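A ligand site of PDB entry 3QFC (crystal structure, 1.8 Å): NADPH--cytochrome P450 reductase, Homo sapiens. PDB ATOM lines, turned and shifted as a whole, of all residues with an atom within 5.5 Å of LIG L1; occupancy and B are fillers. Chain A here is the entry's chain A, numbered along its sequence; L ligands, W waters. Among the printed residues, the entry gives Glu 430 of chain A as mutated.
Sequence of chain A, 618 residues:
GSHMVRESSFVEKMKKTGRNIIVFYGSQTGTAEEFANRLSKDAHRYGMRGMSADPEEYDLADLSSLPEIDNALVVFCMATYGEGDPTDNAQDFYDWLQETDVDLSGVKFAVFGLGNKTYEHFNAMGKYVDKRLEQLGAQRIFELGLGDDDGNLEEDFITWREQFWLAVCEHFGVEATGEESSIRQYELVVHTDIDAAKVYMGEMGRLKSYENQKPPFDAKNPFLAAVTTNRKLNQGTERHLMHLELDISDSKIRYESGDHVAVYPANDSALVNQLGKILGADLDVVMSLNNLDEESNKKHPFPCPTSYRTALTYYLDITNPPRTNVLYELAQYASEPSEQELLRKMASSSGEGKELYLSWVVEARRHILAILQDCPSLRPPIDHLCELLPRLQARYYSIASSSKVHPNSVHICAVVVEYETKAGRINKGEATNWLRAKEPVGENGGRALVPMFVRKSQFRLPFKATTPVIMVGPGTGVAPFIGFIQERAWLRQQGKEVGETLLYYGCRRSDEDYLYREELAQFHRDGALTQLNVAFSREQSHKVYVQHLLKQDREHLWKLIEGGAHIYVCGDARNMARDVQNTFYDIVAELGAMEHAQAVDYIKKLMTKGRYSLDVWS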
ATOM      1  N   TYR A 119      12.509  22.723 -25.459  1.00  0.00           N
ATOM      2  CA  TYR A 119      13.617  22.749 -26.412  1.00  0.00           C
ATOM      3  C   TYR A 119      13.664  24.039 -27.232  1.00  0.00           C
ATOM      4  O   TYR A 119      12.669  24.730 -27.387  1.00  0.00           O
ATOM      5  CB  TYR A 119      13.507  21.539 -27.338  1.00  0.00           C
ATOM      6  CG  TYR A 119      13.870  20.256 -26.651  1.00  0.00           C
ATOM      7  CD1 TYR A 119      15.205  19.883 -26.467  1.00  0.00           C
ATOM      8  CD2 TYR A 119      12.883  19.404 -26.165  1.00  0.00           C
ATOM      9  CE1 TYR A 119      15.538  18.697 -25.822  1.00  0.00           C
ATOM     10  CE2 TYR A 119      13.206  18.218 -25.511  1.00  0.00           C
ATOM     11  CZ  TYR A 119      14.530  17.868 -25.345  1.00  0.00           C
ATOM     12  OH  TYR A 119      14.836  16.694 -24.703  1.00  0.00           O
ATOM     13  N   HIS A 260      25.605  10.417 -26.018  1.00  0.00           N
ATOM     14  CA  HIS A 260      24.686   9.779 -25.083  1.00  0.00           C
ATOM     15  C   HIS A 260      24.810   8.262 -25.122  1.00  0.00           C
ATOM     16  O   HIS A 260      25.120   7.670 -26.171  1.00  0.00           O
ATOM     17  CB  HIS A 260      23.241  10.175 -25.390  1.00  0.00           C
ATOM     18  CG  HIS A 260      22.995  11.653 -25.294  1.00  0.00           C
ATOM     19  ND1 HIS A 260      22.583  12.408 -26.378  1.00  0.00           N
ATOM     20  CD2 HIS A 260      23.119  12.522 -24.272  1.00  0.00           C
ATOM     21  CE1 HIS A 260      22.485  13.679 -26.023  1.00  0.00           C
ATOM     22  NE2 HIS A 260      22.809  13.771 -24.745  1.00  0.00           N
ATOM     23  N   THR A 319       5.203   0.718 -16.479  1.00  0.00           N
ATOM     24  CA  THR A 319       5.401   1.751 -15.458  1.00  0.00           C
ATOM     25  C   THR A 319       4.830   3.129 -15.801  1.00  0.00           C
ATOM     26  O   THR A 319       4.471   3.901 -14.902  1.00  0.00           O
ATOM     27  CB  THR A 319       6.892   1.927 -15.135  1.00  0.00           C
ATOM     28  OG1 THR A 319       7.631   2.106 -16.358  1.00  0.00           O
ATOM     29  CG2 THR A 319       7.412   0.707 -14.396  1.00  0.00           C
ATOM     30  N   ARG A 365      -0.170   9.404 -11.306  1.00  0.00           N
ATOM     31  CA  ARG A 365       0.906   8.546 -11.798  1.00  0.00           C
ATOM     32  C   ARG A 365       0.582   7.064 -11.679  1.00  0.00           C
ATOM     33  O   ARG A 365       1.440   6.260 -11.288  1.00  0.00           O
ATOM     34  CB  ARG A 365       2.187   8.832 -11.022  1.00  0.00           C
ATOM     35  CG  ARG A 365       2.706  10.251 -11.158  1.00  0.00           C
ATOM     36  CD  ARG A 365       3.184  10.550 -12.563  1.00  0.00           C
ATOM     37  NE  ARG A 365       3.937  11.801 -12.602  1.00  0.00           N
ATOM     38  CZ  ARG A 365       3.456  12.970 -13.039  1.00  0.00           C
ATOM     39  NH1 ARG A 365       4.237  14.051 -13.025  1.00  0.00           N
ATOM     40  NH2 ARG A 365       2.215  13.059 -13.486  1.00  0.00           N
ATOM     41  N   ARG A 395      16.572   4.308 -22.208  1.00  0.00           N
ATOM     42  CA  ARG A 395      16.708   5.601 -21.529  1.00  0.00           C
ATOM     43  C   ARG A 395      18.093   6.110 -21.910  1.00  0.00           C
ATOM     44  O   ARG A 395      19.039   5.328 -22.036  1.00  0.00           O
ATOM     45  CB  ARG A 395      16.621   5.461 -20.004  1.00  0.00           C
ATOM     46  CG  ARG A 395      15.245   5.669 -19.436  1.00  0.00           C
ATOM     47  CD  ARG A 395      14.260   4.554 -19.802  1.00  0.00           C
ATOM     48  NE  ARG A 395      13.014   4.763 -19.077  1.00  0.00           N
ATOM     49  CZ  ARG A 395      11.844   4.226 -19.402  1.00  0.00           C
ATOM     50  NH1 ARG A 395      10.781   4.502 -18.660  1.00  0.00           N
ATOM     51  NH2 ARG A 395      11.735   3.433 -20.462  1.00  0.00           N
ATOM     52  N   TYR A 396      18.228   7.432 -22.063  1.00  0.00           N
ATOM     53  CA  TYR A 396      19.490   8.037 -22.443  1.00  0.00           C
ATOM     54  C   TYR A 396      20.189   8.722 -21.264  1.00  0.00           C
ATOM     55  O   TYR A 396      19.540   9.328 -20.422  1.00  0.00           O
ATOM     56  CB  TYR A 396      19.264   9.083 -23.530  1.00  0.00           C
ATOM     57  CG  TYR A 396      18.514   8.570 -24.745  1.00  0.00           C
ATOM     58  CD1 TYR A 396      19.073   7.596 -25.574  1.00  0.00           C
ATOM     59  CD2 TYR A 396      17.243   9.058 -25.062  1.00  0.00           C
ATOM     60  CE1 TYR A 396      18.386   7.123 -26.690  1.00  0.00           C
ATOM     61  CE2 TYR A 396      16.548   8.589 -26.178  1.00  0.00           C
ATOM     62  CZ  TYR A 396      17.130   7.621 -26.990  1.00  0.00           C
ATOM     63  OH  TYR A 396      16.430   7.146 -28.087  1.00  0.00           O
ATOM     64  N   TYR A 397      21.512   8.614 -21.219  1.00  0.00           N
ATOM     65  CA  TYR A 397      22.310   9.250 -20.171  1.00  0.00           C
ATOM     66  C   TYR A 397      23.474   9.971 -20.837  1.00  0.00           C
ATOM     67  O   TYR A 397      24.005   9.511 -21.843  1.00  0.00           O
ATOM     68  CB  TYR A 397      22.799   8.210 -19.174  1.00  0.00           C
ATOM     69  CG  TYR A 397      21.643   7.626 -18.392  1.00  0.00           C
ATOM     70  CD1 TYR A 397      21.095   8.307 -17.316  1.00  0.00           C
ATOM     71  CD2 TYR A 397      20.996   6.468 -18.835  1.00  0.00           C
ATOM     72  CE1 TYR A 397      19.919   7.869 -16.688  1.00  0.00           C
ATOM     73  CE2 TYR A 397      19.830   6.023 -18.229  1.00  0.00           C
ATOM     74  CZ  TYR A 397      19.294   6.727 -17.164  1.00  0.00           C
ATOM     75  OH  TYR A 397      18.094   6.319 -16.618  1.00  0.00           O
ATOM     76  N   SER A 398      23.855  11.121 -20.294  1.00  0.00           N
ATOM     77  CA  SER A 398      24.962  11.855 -20.873  1.00  0.00           C
ATOM     78  C   SER A 398      26.253  11.190 -20.444  1.00  0.00           C
ATOM     79  O   SER A 398      26.540  11.134 -19.249  1.00  0.00           O
ATOM     80  CB  SER A 398      24.906  13.317 -20.400  1.00  0.00           C
ATOM     81  OG  SER A 398      23.653  13.888 -20.742  1.00  0.00           O
ATOM     82  N   CYS A 413      26.284   9.182 -14.817  1.00  0.00           N
ATOM     83  CA  CYS A 413      26.018   9.911 -13.570  1.00  0.00           C
ATOM     84  C   CYS A 413      24.502  10.042 -13.554  1.00  0.00           C
ATOM     85  O   CYS A 413      23.920  10.736 -14.384  1.00  0.00           O
ATOM     86  CB  CYS A 413      26.643  11.298 -13.586  1.00  0.00           C
ATOM     87  SG  CYS A 413      26.089  12.277 -12.170  1.00  0.00           S
ATOM     88  N   ALA A 414      23.835   9.378 -12.614  1.00  0.00           N
ATOM     89  CA  ALA A 414      22.381   9.426 -12.598  1.00  0.00           C
ATOM     90  C   ALA A 414      21.772   9.519 -11.205  1.00  0.00           C
ATOM     91  O   ALA A 414      22.363   9.070 -10.216  1.00  0.00           O
ATOM     92  CB  ALA A 414      21.819   8.183 -13.302  1.00  0.00           C
ATOM     93  N   VAL A 415      20.578  10.101 -11.159  1.00  0.00           N
ATOM     94  CA  VAL A 415      19.832  10.227  -9.913  1.00  0.00           C
ATOM     95  C   VAL A 415      18.654   9.252 -10.015  1.00  0.00           C
ATOM     96  O   VAL A 415      17.939   9.223 -11.030  1.00  0.00           O
ATOM     97  CB  VAL A 415      19.296  11.669  -9.710  1.00  0.00           C
ATOM     98  CG1 VAL A 415      18.454  12.105 -10.905  1.00  0.00           C
ATOM     99  CG2 VAL A 415      18.489  11.738  -8.430  1.00  0.00           C
ATOM    100  N   VAL A 417      15.045   7.727  -9.539  1.00  0.00           N
ATOM    101  CA  VAL A 417      13.690   8.239  -9.400  1.00  0.00           C
ATOM    102  C   VAL A 417      12.933   7.334  -8.422  1.00  0.00           C
ATOM    103  O   VAL A 417      12.892   6.132  -8.597  1.00  0.00           O
ATOM    104  CB  VAL A 417      12.955   8.245 -10.760  1.00  0.00           C
ATOM    105  CG1 VAL A 417      11.494   8.578 -10.578  1.00  0.00           C
ATOM    106  CG2 VAL A 417      13.604   9.260 -11.697  1.00  0.00           C
ATOM    107  N   TYR A 419       9.452   8.023  -5.600  1.00  0.00           N
ATOM    108  CA  TYR A 419       8.570   8.978  -4.943  1.00  0.00           C
ATOM    109  C   TYR A 419       7.226   8.358  -4.585  1.00  0.00           C
ATOM    110  O   TYR A 419       6.839   7.321  -5.117  1.00  0.00           O
ATOM    111  CB  TYR A 419       8.307  10.166  -5.880  1.00  0.00           C
ATOM    112  CG  TYR A 419       7.682   9.766  -7.195  1.00  0.00           C
ATOM    113  CD1 TYR A 419       8.452   9.199  -8.212  1.00  0.00           C
ATOM    114  CD2 TYR A 419       6.310   9.926  -7.416  1.00  0.00           C
ATOM    115  CE1 TYR A 419       7.870   8.795  -9.412  1.00  0.00           C
ATOM    116  CE2 TYR A 419       5.716   9.517  -8.620  1.00  0.00           C
ATOM    117  CZ  TYR A 419       6.498   8.959  -9.610  1.00  0.00           C
ATOM    118  OH  TYR A 419       5.917   8.560 -10.798  1.00  0.00           O
ATOM    119  N   LYS A 428       8.867   3.667  -8.696  1.00  0.00           N
ATOM    120  CA  LYS A 428      10.310   3.574  -8.823  1.00  0.00           C
ATOM    121  C   LYS A 428      10.687   3.732 -10.290  1.00  0.00           C
ATOM    122  O   LYS A 428      10.084   3.100 -11.167  1.00  0.00           O
ATOM    123  CB  LYS A 428      10.803   2.228  -8.295  1.00  0.00           C
ATOM    124  CG  LYS A 428      10.670   2.057  -6.789  1.00  0.00           C
ATOM    125  CD  LYS A 428      11.192   0.707  -6.374  1.00  0.00           C
ATOM    126  CE  LYS A 428      11.041   0.468  -4.881  1.00  0.00           C
ATOM    127  NZ  LYS A 428      11.426  -0.934  -4.542  1.00  0.00           N
ATOM    128  N   GLY A 429      11.660   4.597 -10.552  1.00  0.00           N
ATOM    129  CA  GLY A 429      12.089   4.845 -11.918  1.00  0.00           C
ATOM    130  C   GLY A 429      12.513   3.554 -12.581  1.00  0.00           C
ATOM    131  O   GLY A 429      13.305   2.802 -12.040  1.00  0.00           O
ATOM    132  N   GLU A 430      11.985   3.319 -13.774  1.00  0.00           N
ATOM    133  CA  GLU A 430      12.261   2.114 -14.561  1.00  0.00           C
ATOM    134  C   GLU A 430      13.740   1.773 -14.741  1.00  0.00           C
ATOM    135  O   GLU A 430      14.205   0.715 -14.307  1.00  0.00           O
ATOM    136  CB  GLU A 430      11.591   2.286 -15.944  1.00  0.00           C
ATOM    137  CG  GLU A 430      11.961   1.241 -16.983  1.00  0.00           C
ATOM    138  CD  GLU A 430      11.456  -0.130 -16.627  1.00  0.00           C
ATOM    139  OE1 GLU A 430      10.528  -0.221 -15.792  1.00  0.00           O
ATOM    140  OE2 GLU A 430      11.997  -1.118 -17.188  1.00  0.00           O
ATOM    141  N   ALA A 431      14.475   2.672 -15.374  1.00  0.00           N
ATOM    142  CA  ALA A 431      15.880   2.421 -15.619  1.00  0.00           C
ATOM    143  C   ALA A 431      16.792   2.678 -14.422  1.00  0.00           C
ATOM    144  O   ALA A 431      17.740   1.916 -14.211  1.00  0.00           O
ATOM    145  CB  ALA A 431      16.355   3.241 -16.821  1.00  0.00           C
ATOM    146  N   THR A 432      16.521   3.721 -13.637  1.00  0.00           N
ATOM    147  CA  THR A 432      17.394   4.024 -12.520  1.00  0.00           C
ATOM    148  C   THR A 432      17.329   3.028 -11.365  1.00  0.00           C
ATOM    149  O   THR A 432      18.344   2.712 -10.767  1.00  0.00           O
ATOM    150  CB  THR A 432      17.188   5.476 -12.008  1.00  0.00           C
ATOM    151  OG1 THR A 432      15.815   5.700 -11.636  1.00  0.00           O
ATOM    152  CG2 THR A 432      17.581   6.453 -13.108  1.00  0.00           C
ATOM    153  N   ASN A 433      16.142   2.498 -11.085  1.00  0.00           N
ATOM    154  CA  ASN A 433      16.022   1.511 -10.013  1.00  0.00           C
ATOM    155  C   ASN A 433      16.745   0.239 -10.478  1.00  0.00           C
ATOM    156  O   ASN A 433      17.368  -0.470  -9.685  1.00  0.00           O
ATOM    157  CB  ASN A 433      14.538   1.200  -9.745  1.00  0.00           C
ATOM    158  CG  ASN A 433      14.342   0.229  -8.601  1.00  0.00           C
ATOM    159  OD1 ASN A 433      13.792  -0.859  -8.790  1.00  0.00           O
ATOM    160  ND2 ASN A 433      14.779   0.605  -7.409  1.00  0.00           N
ATOM    161  N   THR A 476      22.710  16.543 -11.846  1.00  0.00           N
ATOM    162  CA  THR A 476      23.202  15.546 -12.781  1.00  0.00           C
ATOM    163  C   THR A 476      23.601  16.173 -14.119  1.00  0.00           C
ATOM    164  O   THR A 476      24.183  15.512 -14.980  1.00  0.00           O
ATOM    165  CB  THR A 476      22.147  14.425 -13.026  1.00  0.00           C
ATOM    166  OG1 THR A 476      20.873  15.008 -13.316  1.00  0.00           O
ATOM    167  CG2 THR A 476      22.049  13.546 -11.780  1.00  0.00           C
ATOM    168  N   ALA A 479      27.178  15.808 -15.508  1.00  0.00           N
ATOM    169  CA  ALA A 479      27.650  14.614 -16.207  1.00  0.00           C
ATOM    170  C   ALA A 479      28.615  14.743 -17.395  1.00  0.00           C
ATOM    171  O   ALA A 479      29.749  14.269 -17.327  1.00  0.00           O
ATOM    172  CB  ALA A 479      26.445  13.764 -16.608  1.00  0.00           C
ATOM    173  N   ASP A 615      22.337  20.380 -23.740  1.00  0.00           N
ATOM    174  CA  ASP A 615      22.111  18.942 -23.512  1.00  0.00           C
ATOM    175  C   ASP A 615      21.195  18.978 -22.298  1.00  0.00           C
ATOM    176  O   ASP A 615      21.614  18.711 -21.178  1.00  0.00           O
ATOM    177  CB  ASP A 615      23.407  18.196 -23.179  1.00  0.00           C
ATOM    178  CG  ASP A 615      23.163  16.703 -22.908  1.00  0.00           C
ATOM    179  OD1 ASP A 615      24.067  16.039 -22.329  1.00  0.00           O
ATOM    180  OD2 ASP A 615      22.096  16.193 -23.266  1.00  0.00           O
ATOM    181  N   VAL A 616      19.938  19.368 -22.523  1.00  0.00           N
ATOM    182  CA  VAL A 616      18.999  19.454 -21.416  1.00  0.00           C
ATOM    183  C   VAL A 616      17.855  18.487 -21.604  1.00  0.00           C
ATOM    184  O   VAL A 616      17.574  18.060 -22.713  1.00  0.00           O
ATOM    185  CB  VAL A 616      18.492  20.902 -21.258  1.00  0.00           C
ATOM    186  CG1 VAL A 616      19.677  21.790 -20.935  1.00  0.00           C
ATOM    187  CG2 VAL A 616      17.777  21.389 -22.517  1.00  0.00           C
ATOM    188  N   TRP A 617      17.202  18.132 -20.498  1.00  0.00           N
ATOM    189  CA  TRP A 617      16.117  17.153 -20.538  1.00  0.00           C
ATOM    190  C   TRP A 617      15.153  17.319 -19.371  1.00  0.00           C
ATOM    191  O   TRP A 617      15.357  18.141 -18.494  1.00  0.00           O
ATOM    192  CB  TRP A 617      16.713  15.746 -20.506  1.00  0.00           C
ATOM    193  CG  TRP A 617      17.459  15.455 -19.226  1.00  0.00           C
ATOM    194  CD1 TRP A 617      16.919  15.076 -18.028  1.00  0.00           C
ATOM    195  CD2 TRP A 617      18.869  15.599 -19.005  1.00  0.00           C
ATOM    196  NE1 TRP A 617      17.900  14.974 -17.078  1.00  0.00           N
ATOM    197  CE2 TRP A 617      19.105  15.293 -17.638  1.00  0.00           C
ATOM    198  CE3 TRP A 617      19.955  15.948 -19.816  1.00  0.00           C
ATOM    199  CZ2 TRP A 617      20.390  15.324 -17.073  1.00  0.00           C
ATOM    200  CZ3 TRP A 617      21.221  15.988 -19.252  1.00  0.00           C
ATOM    201  CH2 TRP A 617      21.436  15.681 -17.890  1.00  0.00           C
ATOM    202  N   SER A 618      14.112  16.493 -19.379  1.00  0.00           N
ATOM    203  CA  SER A 618      13.095  16.493 -18.324  1.00  0.00           C
ATOM    204  C   SER A 618      12.797  15.037 -18.001  1.00  0.00           C
ATOM    205  O   SER A 618      13.056  14.195 -18.879  1.00  0.00           O
ATOM    206  CB  SER A 618      11.814  17.172 -18.801  1.00  0.00           C
ATOM    207  OG  SER A 618      12.053  18.504 -19.215  1.00  0.00           O
ATOM    208  OXT SER A 618      12.283  14.773 -16.892  1.00  0.00           O
HETATM  209  P1  LIG L   1      10.884   6.675 -15.364  1.00  0.00           P
HETATM  210  O1  LIG L   1      10.324   5.375 -14.893  1.00  0.00           O
HETATM  211  O2  LIG L   1      10.877   6.887 -16.824  1.00  0.00           O
HETATM  212  O3  LIG L   1      10.070   7.735 -14.693  1.00  0.00           O
HETATM  213  C1  LIG L   1      10.271   9.149 -14.890  1.00  0.00           C
HETATM  214  C2  LIG L   1       8.980   9.947 -14.760  1.00  0.00           C
HETATM  215  O4  LIG L   1       8.518   9.849 -13.390  1.00  0.00           O
HETATM  216  C3  LIG L   1       9.117  11.456 -14.987  1.00  0.00           C
HETATM  217  O5  LIG L   1       8.972  11.794 -16.356  1.00  0.00           O
HETATM  218  C4  LIG L   1       7.904  12.010 -14.240  1.00  0.00           C
HETATM  219  O6  LIG L   1       6.641  11.972 -14.962  1.00  0.00           O
HETATM  220  C5  LIG L   1       7.846  11.069 -13.025  1.00  0.00           C
HETATM  221  N1  LIG L   1       8.461  11.579 -11.776  1.00  0.00           N
HETATM  222  C6  LIG L   1       9.766  11.638 -11.305  1.00  0.00           C
HETATM  223  N2  LIG L   1       9.896  12.199 -10.052  1.00  0.00           N
HETATM  224  C7  LIG L   1       8.610  12.513  -9.710  1.00  0.00           C
HETATM  225  C8  LIG L   1       7.991  13.123  -8.552  1.00  0.00           C
HETATM  226  N3  LIG L   1       8.712  13.523  -7.461  1.00  0.00           N
HETATM  227  N4  LIG L   1       6.598  13.267  -8.612  1.00  0.00           N
HETATM  228  C9  LIG L   1       5.778  12.907  -9.639  1.00  0.00           C
HETATM  229  N5  LIG L   1       6.253  12.319 -10.789  1.00  0.00           N
HETATM  230  C10 LIG L   1       7.689  12.140 -10.773  1.00  0.00           C
HETATM  231  N6  LIG L   1      19.320  11.446 -16.233  1.00  0.00           N
HETATM  232  C11 LIG L   1      20.384  11.388 -15.370  1.00  0.00           C
HETATM  233  O7  LIG L   1      20.168  11.090 -14.195  1.00  0.00           O
HETATM  234  N7  LIG L   1      21.617  11.656 -15.886  1.00  0.00           N
HETATM  235  C12 LIG L   1      21.948  12.006 -17.233  1.00  0.00           C
HETATM  236  O8  LIG L   1      23.123  12.230 -17.572  1.00  0.00           O
HETATM  237  C13 LIG L   1      20.797  12.086 -18.120  1.00  0.00           C
HETATM  238  N8  LIG L   1      21.074  12.446 -19.434  1.00  0.00           N
HETATM  239  C14 LIG L   1      19.974  12.524 -20.278  1.00  0.00           C
HETATM  240  C15 LIG L   1      20.215  12.911 -21.656  1.00  0.00           C
HETATM  241  C16 LIG L   1      19.153  13.005 -22.615  1.00  0.00           C
HETATM  242  C17 LIG L   1      19.448  13.404 -24.052  1.00  0.00           C
HETATM  243  C18 LIG L   1      17.777  12.702 -22.151  1.00  0.00           C
HETATM  244  C19 LIG L   1      16.554  12.763 -23.059  1.00  0.00           C
HETATM  245  C20 LIG L   1      17.515  12.325 -20.839  1.00  0.00           C
HETATM  246  C21 LIG L   1      18.563  12.230 -19.862  1.00  0.00           C
HETATM  247  N9  LIG L   1      18.372  11.840 -18.442  1.00  0.00           N
HETATM  248  C22 LIG L   1      19.481  11.786 -17.578  1.00  0.00           C
HETATM  249  C23 LIG L   1      17.040  11.491 -17.844  1.00  0.00           C
HETATM  250  C24 LIG L   1      17.118   9.909 -18.177  1.00  0.00           C
HETATM  251  O9  LIG L   1      17.069   9.516 -19.630  1.00  0.00           O
HETATM  252  C25 LIG L   1      15.775   9.270 -17.559  1.00  0.00           C
HETATM  253  O10 LIG L   1      14.567   9.941 -18.032  1.00  0.00           O
HETATM  254  C26 LIG L   1      15.712   9.285 -16.016  1.00  0.00           C
HETATM  255  O11 LIG L   1      16.914   8.624 -15.562  1.00  0.00           O
HETATM  256  C27 LIG L   1      14.533   8.656 -15.454  1.00  0.00           C
HETATM  257  O12 LIG L   1      14.213   7.374 -15.989  1.00  0.00           O
HETATM  258  P2  LIG L   1      13.590   6.240 -15.219  1.00  0.00           P
HETATM  259  O13 LIG L   1      14.389   5.830 -14.015  1.00  0.00           O
HETATM  260  O14 LIG L   1      13.435   5.159 -16.223  1.00  0.00           O
HETATM  261  O15 LIG L   1      12.245   6.974 -14.800  1.00  0.00           O
HETATM  262  N1  LG2 L   2      11.215  18.326 -29.210  1.00  0.00           N
HETATM  263  C1  LG2 L   2      11.255  19.505 -29.882  1.00  0.00           C
HETATM  264  O1  LG2 L   2      10.220  20.125 -30.078  1.00  0.00           O
HETATM  265  N2  LG2 L   2      12.463  19.980 -30.312  1.00  0.00           N
HETATM  266  C2  LG2 L   2      13.693  19.331 -30.103  1.00  0.00           C
HETATM  267  O2  LG2 L   2      14.667  19.939 -30.566  1.00  0.00           O
HETATM  268  C3  LG2 L   2      13.669  18.072 -29.387  1.00  0.00           C
HETATM  269  N3  LG2 L   2      14.902  17.408 -29.172  1.00  0.00           N
HETATM  270  C4  LG2 L   2      14.813  16.219 -28.481  1.00  0.00           C
HETATM  271  C5  LG2 L   2      16.083  15.543 -28.240  1.00  0.00           C
HETATM  272  C6  LG2 L   2      16.156  14.323 -27.555  1.00  0.00           C
HETATM  273  C7  LG2 L   2      17.553  13.722 -27.382  1.00  0.00           C
HETATM  274  C8  LG2 L   2      14.912  13.689 -27.031  1.00  0.00           C
HETATM  275  C9  LG2 L   2      14.888  12.342 -26.266  1.00  0.00           C
HETATM  276  C10 LG2 L   2      13.693  14.312 -27.244  1.00  0.00           C
HETATM  277  C11 LG2 L   2      13.580  15.584 -27.965  1.00  0.00           C
HETATM  278  N4  LG2 L   2      12.319  16.324 -28.229  1.00  0.00           N
HETATM  279  C12 LG2 L   2      12.362  17.620 -28.972  1.00  0.00           C
HETATM  280  C13 LG2 L   2      11.062  15.773 -27.757  1.00  0.00           C
HETATM  281  C14 LG2 L   2      10.417  14.675 -28.661  1.00  0.00           C
HETATM  282  O3  LG2 L   2      10.237  15.212 -30.002  1.00  0.00           O
HETATM  283  C15 LG2 L   2       9.120  14.139 -28.035  1.00  0.00           C
HETATM  284  O4  LG2 L   2       9.524  13.493 -26.804  1.00  0.00           O
HETATM  285  C16 LG2 L   2       8.456  13.088 -28.982  1.00  0.00           C
HETATM  286  O5  LG2 L   2       7.247  12.667 -28.272  1.00  0.00           O
HETATM  287  C17 LG2 L   2       9.281  11.848 -29.192  1.00  0.00           C
HETATM  288  O6  LG2 L   2       8.643  10.927 -30.149  1.00  0.00           O
HETATM  289  P1  LG2 L   2       9.169   9.480 -30.389  1.00  0.00           P
HETATM  290  O7  LG2 L   2       8.893   8.612 -29.189  1.00  0.00           O
HETATM  291  O8  LG2 L   2      10.576   9.512 -30.838  1.00  0.00           O
HETATM  292  O9  LG2 L   2       8.268   9.001 -31.467  1.00  0.00           O
HETATM  293  O   HOH W   1       4.919   9.768 -15.643  1.00  0.00           O
HETATM  294  O   HOH W   2      14.294  11.399 -20.340  1.00  0.00           O
HETATM  295  O   HOH W   3      13.248  11.848 -16.802  1.00  0.00           O
HETATM  296  O   HOH W   4       8.646   8.119 -18.050  1.00  0.00           O
HETATM  297  O   HOH W   5      10.838  10.669 -18.677  1.00  0.00           O
HETATM  298  O   HOH W   6      12.337   8.426 -18.551  1.00  0.00           O
HETATM  299  O   HOH W   7      25.184  10.224 -17.116  1.00  0.00           O
HETATM  300  O   HOH W   8      15.690   8.953 -21.837  1.00  0.00           O
HETATM  301  O   HOH W   9       8.274  10.563 -18.458  1.00  0.00           O
HETATM  302  O   HOH W  10      17.655  10.146 -13.579  1.00  0.00           O
HETATM  303  O   HOH W  11       8.101   4.624 -16.465  1.00  0.00           O
HETATM  304  O   HOH W  12       8.528   4.817 -12.840  1.00  0.00           O
HETATM  305  O   HOH W  13       6.037  13.595 -16.795  1.00  0.00           O
HETATM  306  O   HOH W  14       7.656   7.347 -12.502  1.00  0.00           O
HETATM  307  O   HOH W  15       4.831  12.888  -6.097  1.00  0.00           O
HETATM  308  O   HOH W  16       9.558  14.227 -17.090  1.00  0.00           O
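NE of Arg 365 sits at hydrogen-bond distance from N5 of LIG L1 (3.0 Å).
The backbone NH (N) of Ala 431 lies within hydrogen-bond range of an oxygen (O14) of LIG L1 (2.8 Å).
O13 of LIG L1 is in hydrogen-bond range of N of Thr 432 (3.0 Å).
N of Tyr 396 sits at hydrogen-bond distance from O9 of LIG L1 (3.4 Å).
The guanidinium group of Arg 395 lies within salt-bridge range of an oxygen (O14) of LIG L1.
The side-chain hydroxyl (OH) of Tyr 397 lies within hydrogen-bond range of an oxygen (O11) of LIG L1.
O of Tyr 396 sits at hydrogen-bond distance from O9 of LIG L1 (2.6 Å).
The backbone NH (N) of Ser 398 sits at hydrogen-bond distance from an oxygen (O8) of LIG L1, at 3.0 Å.
The backbone NH of Glu 430 lies within hydrogen-bond range of an oxygen (O1) of LIG L1 (2.9 Å).
The backbone carbonyl oxygen of Cys 413 is in hydrogen-bond range of a nitrogen (N7) of LIG L1 (2.9 Å).
N8 of LIG L1 sits at hydrogen-bond distance from OG of Ser 398 (3.2 Å).
The backbone NH of Val 415 sits at hydrogen-bond distance from an oxygen (O7) of LIG L1, at 3.2 Å.
OG1 of Thr 432 sits at hydrogen-bond distance from O13 of LIG L1 (2.8 Å).
NE2 of His 260 sits at hydrogen-bond distance from OD2 of Asp 615, at 2.9 Å.
The side-chain hydroxyl of Thr 432 sits at hydrogen-bond distance from the backbone NH of Val 417 (3.0 Å).
N of Gly 429 sits at hydrogen-bond distance from O of Val 417 (2.8 Å).
The side-chain carboxylate (OD1) of Asp 615 is in hydrogen-bond range of the side-chain hydroxyl (OG) of Ser 398.
The indole nitrogen of Trp 617 lies close to a nitrogen (N9) of LIG L1, 3.5 Å away.
Merely in contact with LIG L1: His 260 (3.5 Å), Ala 414 (3.2 Å), Val 417 (3.6 Å), Tyr 419 (3.5 Å), Gly 429 (3.3 Å), Thr 476 (3.9 Å), Ala 479 (3.8 Å) and Asp 615 (3.9 Å).
Hydrophobic or aromatic side chains within 4 Å of LIG L1: His 260, Tyr 397, Ala 414, Val 415, Val 417, Tyr 419, Ala 431, Ala 479 and Trp 617.
Within 4 Å of LIG L1: His 260, Arg 365, Arg 395, Tyr 396, Tyr 397, Ser 398, Cys 413, Ala 414, Val 415, Val 417, Tyr 419, Gly 429, Glu 430, Ala 431, Thr 432, Thr 476, Ala 479, Asp 615 and Trp 617.
The nearest printed residue that does not touch LIG L1 is Lys 428 (4.4 Å).
Water W10 bridges an oxygen (O11) of LIG L1 (2.6 Å) and the backbone carbonyl oxygen of Val 415 (2.7 Å).
Water W16 lies within hydrogen-bond range of an oxygen (O5) of LIG L1 (2.6 Å) and the chain-end carboxylate (OXT) of Ser 618 (2.8 Å).
Water W8 bridges O9 of LIG L1 (2.7 Å) and N of Tyr 396 (3.0 Å).
Water W2 bridges O10 of LIG L1 (2.7 Å) and O of Ser 618 (3.4 Å).
Water W12 bridges an oxygen (O1) of LIG L1 (2.8 Å) and the backbone carbonyl oxygen (O) of Lys 428 (2.9 Å).
Water W11 lies within hydrogen-bond range of OG1 of Thr 319, O1 of LIG L1 and NH1 of Arg 395.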
